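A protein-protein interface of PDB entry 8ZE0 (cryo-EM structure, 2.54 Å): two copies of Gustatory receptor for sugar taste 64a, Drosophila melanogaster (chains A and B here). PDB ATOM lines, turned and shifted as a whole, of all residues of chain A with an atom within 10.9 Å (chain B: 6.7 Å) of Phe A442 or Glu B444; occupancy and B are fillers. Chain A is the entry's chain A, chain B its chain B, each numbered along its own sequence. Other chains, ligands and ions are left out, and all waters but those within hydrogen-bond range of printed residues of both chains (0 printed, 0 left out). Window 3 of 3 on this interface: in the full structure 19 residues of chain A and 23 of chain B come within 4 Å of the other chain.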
ATOM      1  N   THR A 125       3.403   7.314  -7.996  1.00  0.00           N
ATOM      2  CA  THR A 125       4.218   7.221  -9.198  1.00  0.00           C
ATOM      3  C   THR A 125       3.524   6.300 -10.200  1.00  0.00           C
ATOM      4  O   THR A 125       2.395   5.854  -9.989  1.00  0.00           O
ATOM      5  CB  THR A 125       5.627   6.716  -8.872  1.00  0.00           C
ATOM      6  OG1 THR A 125       5.646   5.283  -8.921  1.00  0.00           O
ATOM      7  CG2 THR A 125       6.060   7.176  -7.487  1.00  0.00           C
ATOM      8  N   ALA A 126       4.215   6.018 -11.305  1.00  0.00           N
ATOM      9  CA  ALA A 126       3.696   5.091 -12.301  1.00  0.00           C
ATOM     10  C   ALA A 126       3.967   3.635 -11.949  1.00  0.00           C
ATOM     11  O   ALA A 126       3.442   2.743 -12.625  1.00  0.00           O
ATOM     12  CB  ALA A 126       4.291   5.405 -13.676  1.00  0.00           C
ATOM     13  N   LYS A 127       4.765   3.374 -10.914  1.00  0.00           N
ATOM     14  CA  LYS A 127       5.108   2.020 -10.496  1.00  0.00           C
ATOM     15  C   LYS A 127       4.218   1.514  -9.366  1.00  0.00           C
ATOM     16  O   LYS A 127       3.619   0.442  -9.481  1.00  0.00           O
ATOM     17  CB  LYS A 127       6.579   1.964 -10.064  1.00  0.00           C
ATOM     18  CG  LYS A 127       7.314   0.716 -10.513  1.00  0.00           C
ATOM     19  CD  LYS A 127       7.781   0.844 -11.953  1.00  0.00           C
ATOM     20  CE  LYS A 127       8.909  -0.126 -12.253  1.00  0.00           C
ATOM     21  NZ  LYS A 127       9.213  -0.189 -13.709  1.00  0.00           N
ATOM     22  N   CYS A 335       0.475  -4.424 -20.297  1.00  0.00           N
ATOM     23  CA  CYS A 335       1.451  -3.377 -20.578  1.00  0.00           C
ATOM     24  C   CYS A 335       2.399  -3.178 -19.402  1.00  0.00           C
ATOM     25  O   CYS A 335       3.613  -3.040 -19.592  1.00  0.00           O
ATOM     26  CB  CYS A 335       0.735  -2.071 -20.920  1.00  0.00           C
ATOM     27  SG  CYS A 335      -0.107  -2.080 -22.519  1.00  0.00           S
ATOM     28  N   LEU A 338       4.833  -6.207 -19.278  1.00  0.00           N
ATOM     29  CA  LEU A 338       5.803  -6.151 -20.365  1.00  0.00           C
ATOM     30  C   LEU A 338       6.789  -5.007 -20.170  1.00  0.00           C
ATOM     31  O   LEU A 338       7.931  -5.085 -20.637  1.00  0.00           O
ATOM     32  CB  LEU A 338       5.085  -6.023 -21.706  1.00  0.00           C
ATOM     33  CG  LEU A 338       4.416  -7.309 -22.192  1.00  0.00           C
ATOM     34  CD1 LEU A 338       3.679  -7.074 -23.497  1.00  0.00           C
ATOM     35  CD2 LEU A 338       5.444  -8.420 -22.345  1.00  0.00           C
ATOM     36  N   LEU A 339       6.364  -3.935 -19.498  1.00  0.00           N
ATOM     37  CA  LEU A 339       7.296  -2.879 -19.120  1.00  0.00           C
ATOM     38  C   LEU A 339       8.271  -3.364 -18.053  1.00  0.00           C
ATOM     39  O   LEU A 339       9.461  -3.031 -18.092  1.00  0.00           O
ATOM     40  CB  LEU A 339       6.514  -1.659 -18.635  1.00  0.00           C
ATOM     41  CG  LEU A 339       7.027  -0.252 -18.952  1.00  0.00           C
ATOM     42  CD1 LEU A 339       5.970   0.777 -18.593  1.00  0.00           C
ATOM     43  CD2 LEU A 339       8.311   0.035 -18.203  1.00  0.00           C
ATOM     44  N   ASN A 340       7.786  -4.159 -17.098  1.00  0.00           N
ATOM     45  CA  ASN A 340       8.609  -4.638 -15.992  1.00  0.00           C
ATOM     46  C   ASN A 340       9.420  -5.886 -16.330  1.00  0.00           C
ATOM     47  O   ASN A 340      10.177  -6.360 -15.476  1.00  0.00           O
ATOM     48  CB  ASN A 340       7.728  -4.923 -14.773  1.00  0.00           C
ATOM     49  CG  ASN A 340       7.947  -3.935 -13.649  1.00  0.00           C
ATOM     50  OD1 ASN A 340       8.481  -2.847 -13.862  1.00  0.00           O
ATOM     51  ND2 ASN A 340       7.529  -4.304 -12.444  1.00  0.00           N
ATOM     52  N   PHE A 342      11.952  -6.385 -18.201  1.00  0.00           N
ATOM     53  CA  PHE A 342      13.396  -6.256 -18.378  1.00  0.00           C
ATOM     54  C   PHE A 342      14.188  -6.101 -17.081  1.00  0.00           C
ATOM     55  O   PHE A 342      15.411  -6.278 -17.111  1.00  0.00           O
ATOM     56  CB  PHE A 342      13.734  -5.085 -19.306  1.00  0.00           C
ATOM     57  CG  PHE A 342      13.588  -5.401 -20.767  1.00  0.00           C
ATOM     58  CD1 PHE A 342      14.701  -5.722 -21.521  1.00  0.00           C
ATOM     59  CD2 PHE A 342      12.355  -5.348 -21.394  1.00  0.00           C
ATOM     60  CE1 PHE A 342      14.592  -6.004 -22.866  1.00  0.00           C
ATOM     61  CE2 PHE A 342      12.237  -5.632 -22.744  1.00  0.00           C
ATOM     62  CZ  PHE A 342      13.360  -5.959 -23.480  1.00  0.00           C
ATOM     63  N   ASN A 343      13.553  -5.780 -15.955  1.00  0.00           N
ATOM     64  CA  ASN A 343      14.333  -5.591 -14.740  1.00  0.00           C
ATOM     65  C   ASN A 343      14.820  -6.931 -14.193  1.00  0.00           C
ATOM     66  O   ASN A 343      14.413  -8.009 -14.638  1.00  0.00           O
ATOM     67  CB  ASN A 343      13.532  -4.845 -13.676  1.00  0.00           C
ATOM     68  CG  ASN A 343      12.503  -3.908 -14.266  1.00  0.00           C
ATOM     69  OD1 ASN A 343      11.318  -4.224 -14.321  1.00  0.00           O
ATOM     70  ND2 ASN A 343      12.955  -2.745 -14.719  1.00  0.00           N
ATOM     71  N   THR A 434       3.308  -1.449 -29.872  1.00  0.00           N
ATOM     72  CA  THR A 434       3.599  -0.026 -30.034  1.00  0.00           C
ATOM     73  C   THR A 434       3.702   0.680 -28.685  1.00  0.00           C
ATOM     74  O   THR A 434       4.619   1.484 -28.462  1.00  0.00           O
ATOM     75  CB  THR A 434       2.524   0.633 -30.899  1.00  0.00           C
ATOM     76  OG1 THR A 434       2.428  -0.055 -32.152  1.00  0.00           O
ATOM     77  CG2 THR A 434       2.862   2.094 -31.153  1.00  0.00           C
ATOM     78  N   TYR A 435       2.773   0.388 -27.772  1.00  0.00           N
ATOM     79  CA  TYR A 435       2.793   1.023 -26.459  1.00  0.00           C
ATOM     80  C   TYR A 435       4.048   0.645 -25.685  1.00  0.00           C
ATOM     81  O   TYR A 435       4.646   1.489 -25.010  1.00  0.00           O
ATOM     82  CB  TYR A 435       1.542   0.640 -25.667  1.00  0.00           C
ATOM     83  CG  TYR A 435       0.265   1.304 -26.140  1.00  0.00           C
ATOM     84  CD1 TYR A 435       0.261   2.153 -27.239  1.00  0.00           C
ATOM     85  CD2 TYR A 435      -0.937   1.081 -25.482  1.00  0.00           C
ATOM     86  CE1 TYR A 435      -0.906   2.758 -27.670  1.00  0.00           C
ATOM     87  CE2 TYR A 435      -2.106   1.682 -25.904  1.00  0.00           C
ATOM     88  CZ  TYR A 435      -2.086   2.519 -26.998  1.00  0.00           C
ATOM     89  OH  TYR A 435      -3.250   3.119 -27.421  1.00  0.00           O
ATOM     90  N   GLU A 436       4.460  -0.623 -25.766  1.00  0.00           N
ATOM     91  CA  GLU A 436       5.688  -1.046 -25.105  1.00  0.00           C
ATOM     92  C   GLU A 436       6.905  -0.366 -25.715  1.00  0.00           C
ATOM     93  O   GLU A 436       7.818   0.049 -24.991  1.00  0.00           O
ATOM     94  CB  GLU A 436       5.827  -2.566 -25.180  1.00  0.00           C
ATOM     95  CG  GLU A 436       4.913  -3.307 -24.225  1.00  0.00           C
ATOM     96  CD  GLU A 436       4.946  -2.721 -22.830  1.00  0.00           C
ATOM     97  OE1 GLU A 436       6.032  -2.713 -22.214  1.00  0.00           O
ATOM     98  OE2 GLU A 436       3.890  -2.259 -22.352  1.00  0.00           O
ATOM     99  N   LEU A 437       6.938  -0.243 -27.044  1.00  0.00           N
ATOM    100  CA  LEU A 437       8.051   0.441 -27.692  1.00  0.00           C
ATOM    101  C   LEU A 437       8.141   1.891 -27.238  1.00  0.00           C
ATOM    102  O   LEU A 437       9.241   2.423 -27.047  1.00  0.00           O
ATOM    103  CB  LEU A 437       7.905   0.360 -29.212  1.00  0.00           C
ATOM    104  CG  LEU A 437       8.237  -0.983 -29.863  1.00  0.00           C
ATOM    105  CD1 LEU A 437       7.945  -0.945 -31.355  1.00  0.00           C
ATOM    106  CD2 LEU A 437       9.688  -1.357 -29.607  1.00  0.00           C
ATOM    107  N   VAL A 438       6.994   2.549 -27.064  1.00  0.00           N
ATOM    108  CA  VAL A 438       7.008   3.933 -26.594  1.00  0.00           C
ATOM    109  C   VAL A 438       7.432   4.006 -25.129  1.00  0.00           C
ATOM    110  O   VAL A 438       8.225   4.873 -24.743  1.00  0.00           O
ATOM    111  CB  VAL A 438       5.636   4.593 -26.824  1.00  0.00           C
ATOM    112  CG1 VAL A 438       5.638   6.010 -26.278  1.00  0.00           C
ATOM    113  CG2 VAL A 438       5.296   4.599 -28.305  1.00  0.00           C
ATOM    114  N   LEU A 439       6.916   3.102 -24.290  1.00  0.00           N
ATOM    115  CA  LEU A 439       7.157   3.173 -22.851  1.00  0.00           C
ATOM    116  C   LEU A 439       8.553   2.709 -22.450  1.00  0.00           C
ATOM    117  O   LEU A 439       9.011   3.036 -21.347  1.00  0.00           O
ATOM    118  CB  LEU A 439       6.108   2.346 -22.106  1.00  0.00           C
ATOM    119  CG  LEU A 439       4.731   2.993 -21.955  1.00  0.00           C
ATOM    120  CD1 LEU A 439       3.644   1.932 -21.868  1.00  0.00           C
ATOM    121  CD2 LEU A 439       4.695   3.904 -20.738  1.00  0.00           C
ATOM    122  N   LEU A 440       9.241   1.951 -23.304  1.00  0.00           N
ATOM    123  CA  LEU A 440      10.624   1.613 -22.986  1.00  0.00           C
ATOM    124  C   LEU A 440      11.513   2.851 -22.993  1.00  0.00           C
ATOM    125  O   LEU A 440      12.572   2.852 -22.358  1.00  0.00           O
ATOM    126  CB  LEU A 440      11.153   0.551 -23.949  1.00  0.00           C
ATOM    127  CG  LEU A 440      10.559  -0.853 -23.827  1.00  0.00           C
ATOM    128  CD1 LEU A 440      10.859  -1.677 -25.070  1.00  0.00           C
ATOM    129  CD2 LEU A 440      11.083  -1.546 -22.579  1.00  0.00           C
ATOM    130  N   GLN A 441      11.093   3.920 -23.677  1.00  0.00           N
ATOM    131  CA  GLN A 441      11.770   5.205 -23.518  1.00  0.00           C
ATOM    132  C   GLN A 441      11.719   5.677 -22.070  1.00  0.00           C
ATOM    133  O   GLN A 441      12.726   6.151 -21.530  1.00  0.00           O
ATOM    134  CB  GLN A 441      11.143   6.253 -24.440  1.00  0.00           C
ATOM    135  CG  GLN A 441      11.890   6.497 -25.743  1.00  0.00           C
ATOM    136  CD  GLN A 441      11.878   5.300 -26.668  1.00  0.00           C
ATOM    137  OE1 GLN A 441      10.833   4.909 -27.185  1.00  0.00           O
ATOM    138  NE2 GLN A 441      13.051   4.722 -26.895  1.00  0.00           N
ATOM    139  N   PHE A 442      10.554   5.562 -21.428  1.00  0.00           N
ATOM    140  CA  PHE A 442      10.449   5.894 -20.011  1.00  0.00           C
ATOM    141  C   PHE A 442      11.263   4.928 -19.164  1.00  0.00           C
ATOM    142  O   PHE A 442      11.862   5.322 -18.156  1.00  0.00           O
ATOM    143  CB  PHE A 442       8.988   5.861 -19.570  1.00  0.00           C
ATOM    144  CG  PHE A 442       8.139   6.916 -20.204  1.00  0.00           C
ATOM    145  CD1 PHE A 442       8.162   8.219 -19.741  1.00  0.00           C
ATOM    146  CD2 PHE A 442       7.305   6.598 -21.261  1.00  0.00           C
ATOM    147  CE1 PHE A 442       7.376   9.185 -20.327  1.00  0.00           C
ATOM    148  CE2 PHE A 442       6.516   7.557 -21.849  1.00  0.00           C
ATOM    149  CZ  PHE A 442       6.552   8.851 -21.383  1.00  0.00           C
ATOM    150  N   ASP A 443      11.275   3.652 -19.552  1.00  0.00           N
ATOM    151  CA  ASP A 443      11.939   2.633 -18.742  1.00  0.00           C
ATOM    152  C   ASP A 443      13.459   2.739 -18.812  1.00  0.00           C
ATOM    153  O   ASP A 443      14.150   2.319 -17.876  1.00  0.00           O
ATOM    154  CB  ASP A 443      11.486   1.244 -19.188  1.00  0.00           C
ATOM    155  CG  ASP A 443      12.036   0.141 -18.308  1.00  0.00           C
ATOM    156  OD1 ASP A 443      11.967   0.277 -17.068  1.00  0.00           O
ATOM    157  OD2 ASP A 443      12.533  -0.864 -18.856  1.00  0.00           O
ATOM    158  N   GLU A 444      13.995   3.288 -19.902  1.00  0.00           N
ATOM    159  CA  GLU A 444      15.441   3.299 -20.127  1.00  0.00           C
ATOM    160  C   GLU A 444      16.244   4.021 -19.047  1.00  0.00           C
ATOM    161  O   GLU A 444      17.249   3.457 -18.589  1.00  0.00           O
ATOM    162  CB  GLU A 444      15.725   3.899 -21.512  1.00  0.00           C
ATOM    163  CG  GLU A 444      17.160   3.724 -21.981  1.00  0.00           C
ATOM    164  CD  GLU A 444      17.512   2.275 -22.254  1.00  0.00           C
ATOM    165  OE1 GLU A 444      16.618   1.514 -22.683  1.00  0.00           O
ATOM    166  OE2 GLU A 444      18.682   1.895 -22.040  1.00  0.00           O
ATOM    167  N   PRO A 445      15.891   5.237 -18.608  1.00  0.00           N
ATOM    168  CA  PRO A 445      16.741   5.918 -17.613  1.00  0.00           C
ATOM    169  C   PRO A 445      16.854   5.187 -16.286  1.00  0.00           C
ATOM    170  O   PRO A 445      17.817   5.430 -15.548  1.00  0.00           O
ATOM    171  CB  PRO A 445      16.061   7.285 -17.441  1.00  0.00           C
ATOM    172  CG  PRO A 445      14.669   7.085 -17.920  1.00  0.00           C
ATOM    173  CD  PRO A 445      14.780   6.102 -19.038  1.00  0.00           C
ATOM    174  N   ASN A 446      15.906   4.308 -15.953  1.00  0.00           N
ATOM    175  CA  ASN A 446      16.016   3.545 -14.713  1.00  0.00           C
ATOM    176  C   ASN A 446      17.217   2.608 -14.744  1.00  0.00           C
ATOM    177  O   ASN A 446      17.923   2.460 -13.740  1.00  0.00           O
ATOM    178  CB  ASN A 446      14.729   2.761 -14.461  1.00  0.00           C
ATOM    179  CG  ASN A 446      13.511   3.657 -14.360  1.00  0.00           C
ATOM    180  OD1 ASN A 446      13.599   4.868 -14.563  1.00  0.00           O
ATOM    181  ND2 ASN A 446      12.364   3.066 -14.044  1.00  0.00           N
ATOM    182  N   ARG A 447      17.465   1.969 -15.883  1.00  0.00           N
ATOM    183  CA  ARG A 447      18.585   1.047 -16.020  1.00  0.00           C
ATOM    184  C   ARG A 447      19.745   1.697 -16.765  1.00  0.00           C
ATOM    185  O   ARG A 447      20.515   1.020 -17.447  1.00  0.00           O
ATOM    186  CB  ARG A 447      18.142  -0.225 -16.743  1.00  0.00           C
ATOM    187  CG  ARG A 447      17.087  -1.024 -15.999  1.00  0.00           C
ATOM    188  CD  ARG A 447      16.905  -2.397 -16.618  1.00  0.00           C
ATOM    189  NE  ARG A 447      16.546  -2.304 -18.028  1.00  0.00           N
ATOM    190  CZ  ARG A 447      15.311  -2.129 -18.476  1.00  0.00           C
ATOM    191  NH1 ARG A 447      14.284  -2.032 -17.648  1.00  0.00           N
ATOM    192  NH2 ARG A 447      15.101  -2.049 -19.786  1.00  0.00           N
ATOM    193  N   GLU B 436      -0.309  11.060 -26.429  1.00  0.00           N
ATOM    194  CA  GLU B 436       0.140  11.381 -25.079  1.00  0.00           C
ATOM    195  C   GLU B 436       1.407  10.616 -24.723  1.00  0.00           C
ATOM    196  O   GLU B 436       2.321  11.173 -24.105  1.00  0.00           O
ATOM    197  CB  GLU B 436      -0.970  11.085 -24.073  1.00  0.00           C
ATOM    198  CG  GLU B 436      -2.084  12.112 -24.078  1.00  0.00           C
ATOM    199  CD  GLU B 436      -1.555  13.531 -24.061  1.00  0.00           C
ATOM    200  OE1 GLU B 436      -0.856  13.894 -23.093  1.00  0.00           O
ATOM    201  OE2 GLU B 436      -1.830  14.279 -25.021  1.00  0.00           O
ATOM    202  N   LEU B 437       1.478   9.338 -25.102  1.00  0.00           N
ATOM    203  CA  LEU B 437       2.681   8.557 -24.836  1.00  0.00           C
ATOM    204  C   LEU B 437       3.891   9.162 -25.534  1.00  0.00           C
ATOM    205  O   LEU B 437       4.995   9.179 -24.978  1.00  0.00           O
ATOM    206  CB  LEU B 437       2.476   7.107 -25.274  1.00  0.00           C
ATOM    207  CG  LEU B 437       1.604   6.234 -24.369  1.00  0.00           C
ATOM    208  CD1 LEU B 437       1.402   4.857 -24.984  1.00  0.00           C
ATOM    209  CD2 LEU B 437       2.216   6.122 -22.983  1.00  0.00           C
ATOM    210  N   VAL B 438       3.705   9.661 -26.756  1.00  0.00           N
ATOM    211  CA  VAL B 438       4.815  10.290 -27.468  1.00  0.00           C
ATOM    212  C   VAL B 438       5.185  11.627 -26.829  1.00  0.00           C
ATOM    213  O   VAL B 438       6.369  11.940 -26.659  1.00  0.00           O
ATOM    214  CB  VAL B 438       4.478  10.447 -28.961  1.00  0.00           C
ATOM    215  CG1 VAL B 438       5.610  11.155 -29.684  1.00  0.00           C
ATOM    216  CG2 VAL B 438       4.222   9.087 -29.590  1.00  0.00           C
ATOM    217  N   LEU B 439       4.186  12.434 -26.463  1.00  0.00           N
ATOM    218  CA  LEU B 439       4.438  13.785 -25.967  1.00  0.00           C
ATOM    219  C   LEU B 439       4.951  13.814 -24.532  1.00  0.00           C
ATOM    220  O   LEU B 439       5.528  14.824 -24.110  1.00  0.00           O
ATOM    221  CB  LEU B 439       3.165  14.627 -26.074  1.00  0.00           C
ATOM    222  CG  LEU B 439       2.827  15.152 -27.471  1.00  0.00           C
ATOM    223  CD1 LEU B 439       1.326  15.336 -27.627  1.00  0.00           C
ATOM    224  CD2 LEU B 439       3.562  16.454 -27.748  1.00  0.00           C
ATOM    225  N   LEU B 440       4.752  12.742 -23.764  1.00  0.00           N
ATOM    226  CA  LEU B 440       5.352  12.708 -22.435  1.00  0.00           C
ATOM    227  C   LEU B 440       6.874  12.670 -22.515  1.00  0.00           C
ATOM    228  O   LEU B 440       7.551  13.055 -21.557  1.00  0.00           O
ATOM    229  CB  LEU B 440       4.814  11.528 -21.629  1.00  0.00           C
ATOM    230  CG  LEU B 440       3.348  11.595 -21.197  1.00  0.00           C
ATOM    231  CD1 LEU B 440       2.843  10.223 -20.780  1.00  0.00           C
ATOM    232  CD2 LEU B 440       3.169  12.603 -20.072  1.00  0.00           C
ATOM    233  N   GLN B 441       7.431  12.233 -23.649  1.00  0.00           N
ATOM    234  CA  GLN B 441       8.863  12.405 -23.877  1.00  0.00           C
ATOM    235  C   GLN B 441       9.253  13.878 -23.843  1.00  0.00           C
ATOM    236  O   GLN B 441      10.265  14.245 -23.236  1.00  0.00           O
ATOM    237  CB  GLN B 441       9.268  11.782 -25.214  1.00  0.00           C
ATOM    238  CG  GLN B 441       9.877  10.390 -25.121  1.00  0.00           C
ATOM    239  CD  GLN B 441       8.898   9.345 -24.633  1.00  0.00           C
ATOM    240  OE1 GLN B 441       7.926   9.018 -25.315  1.00  0.00           O
ATOM    241  NE2 GLN B 441       9.161   8.798 -23.453  1.00  0.00           N
ATOM    242  N   PHE B 442       8.463  14.736 -24.495  1.00  0.00           N
ATOM    243  CA  PHE B 442       8.708  16.173 -24.424  1.00  0.00           C
ATOM    244  C   PHE B 442       8.481  16.695 -23.014  1.00  0.00           C
ATOM    245  O   PHE B 442       9.195  17.592 -22.549  1.00  0.00           O
ATOM    246  CB  PHE B 442       7.794  16.911 -25.399  1.00  0.00           C
ATOM    247  CG  PHE B 442       8.075  16.614 -26.837  1.00  0.00           C
ATOM    248  CD1 PHE B 442       9.129  17.223 -27.493  1.00  0.00           C
ATOM    249  CD2 PHE B 442       7.273  15.729 -27.536  1.00  0.00           C
ATOM    250  CE1 PHE B 442       9.380  16.947 -28.819  1.00  0.00           C
ATOM    251  CE2 PHE B 442       7.519  15.452 -28.861  1.00  0.00           C
ATOM    252  CZ  PHE B 442       8.573  16.060 -29.501  1.00  0.00           C
ATOM    253  N   ASP B 443       7.474  16.154 -22.327  1.00  0.00           N
ATOM    254  CA  ASP B 443       7.111  16.665 -21.008  1.00  0.00           C
ATOM    255  C   ASP B 443       8.132  16.284 -19.939  1.00  0.00           C
ATOM    256  O   ASP B 443       8.260  16.988 -18.931  1.00  0.00           O
ATOM    257  CB  ASP B 443       5.725  16.155 -20.618  1.00  0.00           C
ATOM    258  CG  ASP B 443       5.229  16.748 -19.316  1.00  0.00           C
ATOM    259  OD1 ASP B 443       5.335  17.980 -19.143  1.00  0.00           O
ATOM    260  OD2 ASP B 443       4.729  15.981 -18.467  1.00  0.00           O
ATOM    261  N   GLU B 444       8.856  15.183 -20.137  1.00  0.00           N
ATOM    262  CA  GLU B 444       9.753  14.656 -19.107  1.00  0.00           C
ATOM    263  C   GLU B 444      10.852  15.621 -18.670  1.00  0.00           C
ATOM    264  O   GLU B 444      11.047  15.776 -17.454  1.00  0.00           O
ATOM    265  CB  GLU B 444      10.351  13.330 -19.598  1.00  0.00           C
ATOM    266  CG  GLU B 444      11.086  12.545 -18.524  1.00  0.00           C
ATOM    267  CD  GLU B 444      10.155  12.020 -17.447  1.00  0.00           C
ATOM    268  OE1 GLU B 444       8.991  11.700 -17.769  1.00  0.00           O
ATOM    269  OE2 GLU B 444      10.588  11.927 -16.281  1.00  0.00           O
ATOM    270  N   PRO B 445      11.603  16.277 -19.563  1.00  0.00           N
ATOM    271  CA  PRO B 445      12.698  17.143 -19.088  1.00  0.00           C
ATOM    272  C   PRO B 445      12.240  18.311 -18.231  1.00  0.00           C
ATOM    273  O   PRO B 445      13.051  18.849 -17.468  1.00  0.00           O
ATOM    274  CB  PRO B 445      13.356  17.630 -20.387  1.00  0.00           C
ATOM    275  CG  PRO B 445      12.323  17.441 -21.438  1.00  0.00           C
ATOM    276  CD  PRO B 445      11.581  16.209 -21.035  1.00  0.00           C
ATOM    277  N   ASN B 446      10.974  18.725 -18.332  1.00  0.00           N
ATOM    278  CA  ASN B 446      10.485  19.805 -17.480  1.00  0.00           C
ATOM    279  C   ASN B 446      10.490  19.396 -16.011  1.00  0.00           C
ATOM    280  O   ASN B 446      10.846  20.198 -15.139  1.00  0.00           O
ATOM    281  CB  ASN B 446       9.082  20.226 -17.915  1.00  0.00           C
ATOM    282  CG  ASN B 446       9.037  20.700 -19.353  1.00  0.00           C
ATOM    283  OD1 ASN B 446      10.035  20.640 -20.071  1.00  0.00           O
ATOM    284  ND2 ASN B 446       7.874  21.178 -19.783  1.00  0.00           N
ATOM    285  N   ARG B 447      10.104  18.159 -15.720  1.00  0.00           N
ATOM    286  CA  ARG B 447      10.068  17.668 -14.348  1.00  0.00           C
ATOM    287  C   ARG B 447      11.271  16.780 -14.049  1.00  0.00           C
ATOM    288  O   ARG B 447      11.191  15.868 -13.226  1.00  0.00           O
ATOM    289  CB  ARG B 447       8.770  16.902 -14.091  1.00  0.00           C
ATOM    290  CG  ARG B 447       7.516  17.748 -14.220  1.00  0.00           C
ATOM    291  CD  ARG B 447       6.304  17.012 -13.679  1.00  0.00           C
ATOM    292  NE  ARG B 447       6.108  15.736 -14.355  1.00  0.00           N
ATOM    293  CZ  ARG B 447       5.466  15.590 -15.506  1.00  0.00           C
ATOM    294  NH1 ARG B 447       4.935  16.625 -16.136  1.00  0.00           N
ATOM    295  NH2 ARG B 447       5.354  14.376 -16.038  1.00  0.00           N
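The backbone carbonyl oxygen (O) of Leu A437 sits close to the side-chain amide oxygen (OE1) of Gln A441 (3.0 Å). OE1 of Gln B441 lies close to O of Leu B437 (3.0 Å).
Among the printed residues, pairs that only touch across the chains: Tyr A435 with Leu B437, Val A438 with Leu B437, Val A438 with Gln B441, Gln A441 with Gln B441, Phe A442 with Leu B437, Phe A442 with Leu B440, Phe A442 with Gln B441 and Phe A442 with Glu B444.
Phe A442 touches four residues of chain B. Glu B444 touches just one residue of chain A: Phe A442. Of chain A, only Phe A442 (3.2 Å) comes within 4 Å of Leu B440. Of the printed residues of chain A, Gln B441 touches Val A438 (3.9 Å), Gln A441 (3.4 Å) and Phe A442 (3.3 Å). Asp B443 touches none of the printed residues of chain A. No residue of chain A comes within 4 Å of Pro B445. No residue of chain A comes within 4 Å of Asn B446. No residue of chain A comes within 4 Å of Arg B447. Of the printed residues of chain B, Val A438 touches Leu B437 (3.5 Å) and Gln B441 (3.9 Å). Of the printed residues of chain A, Leu B437 touches Tyr A435 (3.7 Å), Val A438 (3.5 Å) and Phe A442 (3.8 Å). The nearest residue of chain B that does not touch Phe A442 is Glu B436 (5.5 Å). The nearest printed residue of chain B that does not touch Gln A441 is Leu B437 (6.8 Å).
Of the 12 printed residues of chain B, 4 touch a printed residue of chain A. Printed residues of chain B that touch a printed residue of chain A: Leu B437, Leu B440, Gln B441 and Glu B444. Printed residues of chain A that touch a printed residue of chain B: Tyr A435, Val A438, Gln A441 and Phe A442. Hydrophobic or aromatic side chains of chain A that line the printed part of chain B: Tyr A435, Val A438 and Phe A442. Among the printed residues, 8 pairs touch across the chains. Among the printed residues, no Asp or Glu carboxylate lies within 4 Å of a Lys or Arg side-chain nitrogen of the other chain.
Gln A441 touches its own counterpart, Gln B441. Phe A442 touches Leu B437, but with the chains exchanged Leu A437 does not touch Phe B442 (12.6 Å). Phe A442 touches Gln B441, but with the chains exchanged Gln A441 does not touch Phe B442 (8.9 Å). Phe A442 touches Glu B444, but with the chains exchanged Glu A444 does not touch Phe B442 (13.4 Å). Positions printed for both chains: 436, 437, 438, 439, 440, 441, 442, 443, 444, 445, 446 and 447. Of the 8 pairs that touch across the chains among the printed residues, 1 has its exchanged pair printed and touching as well.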
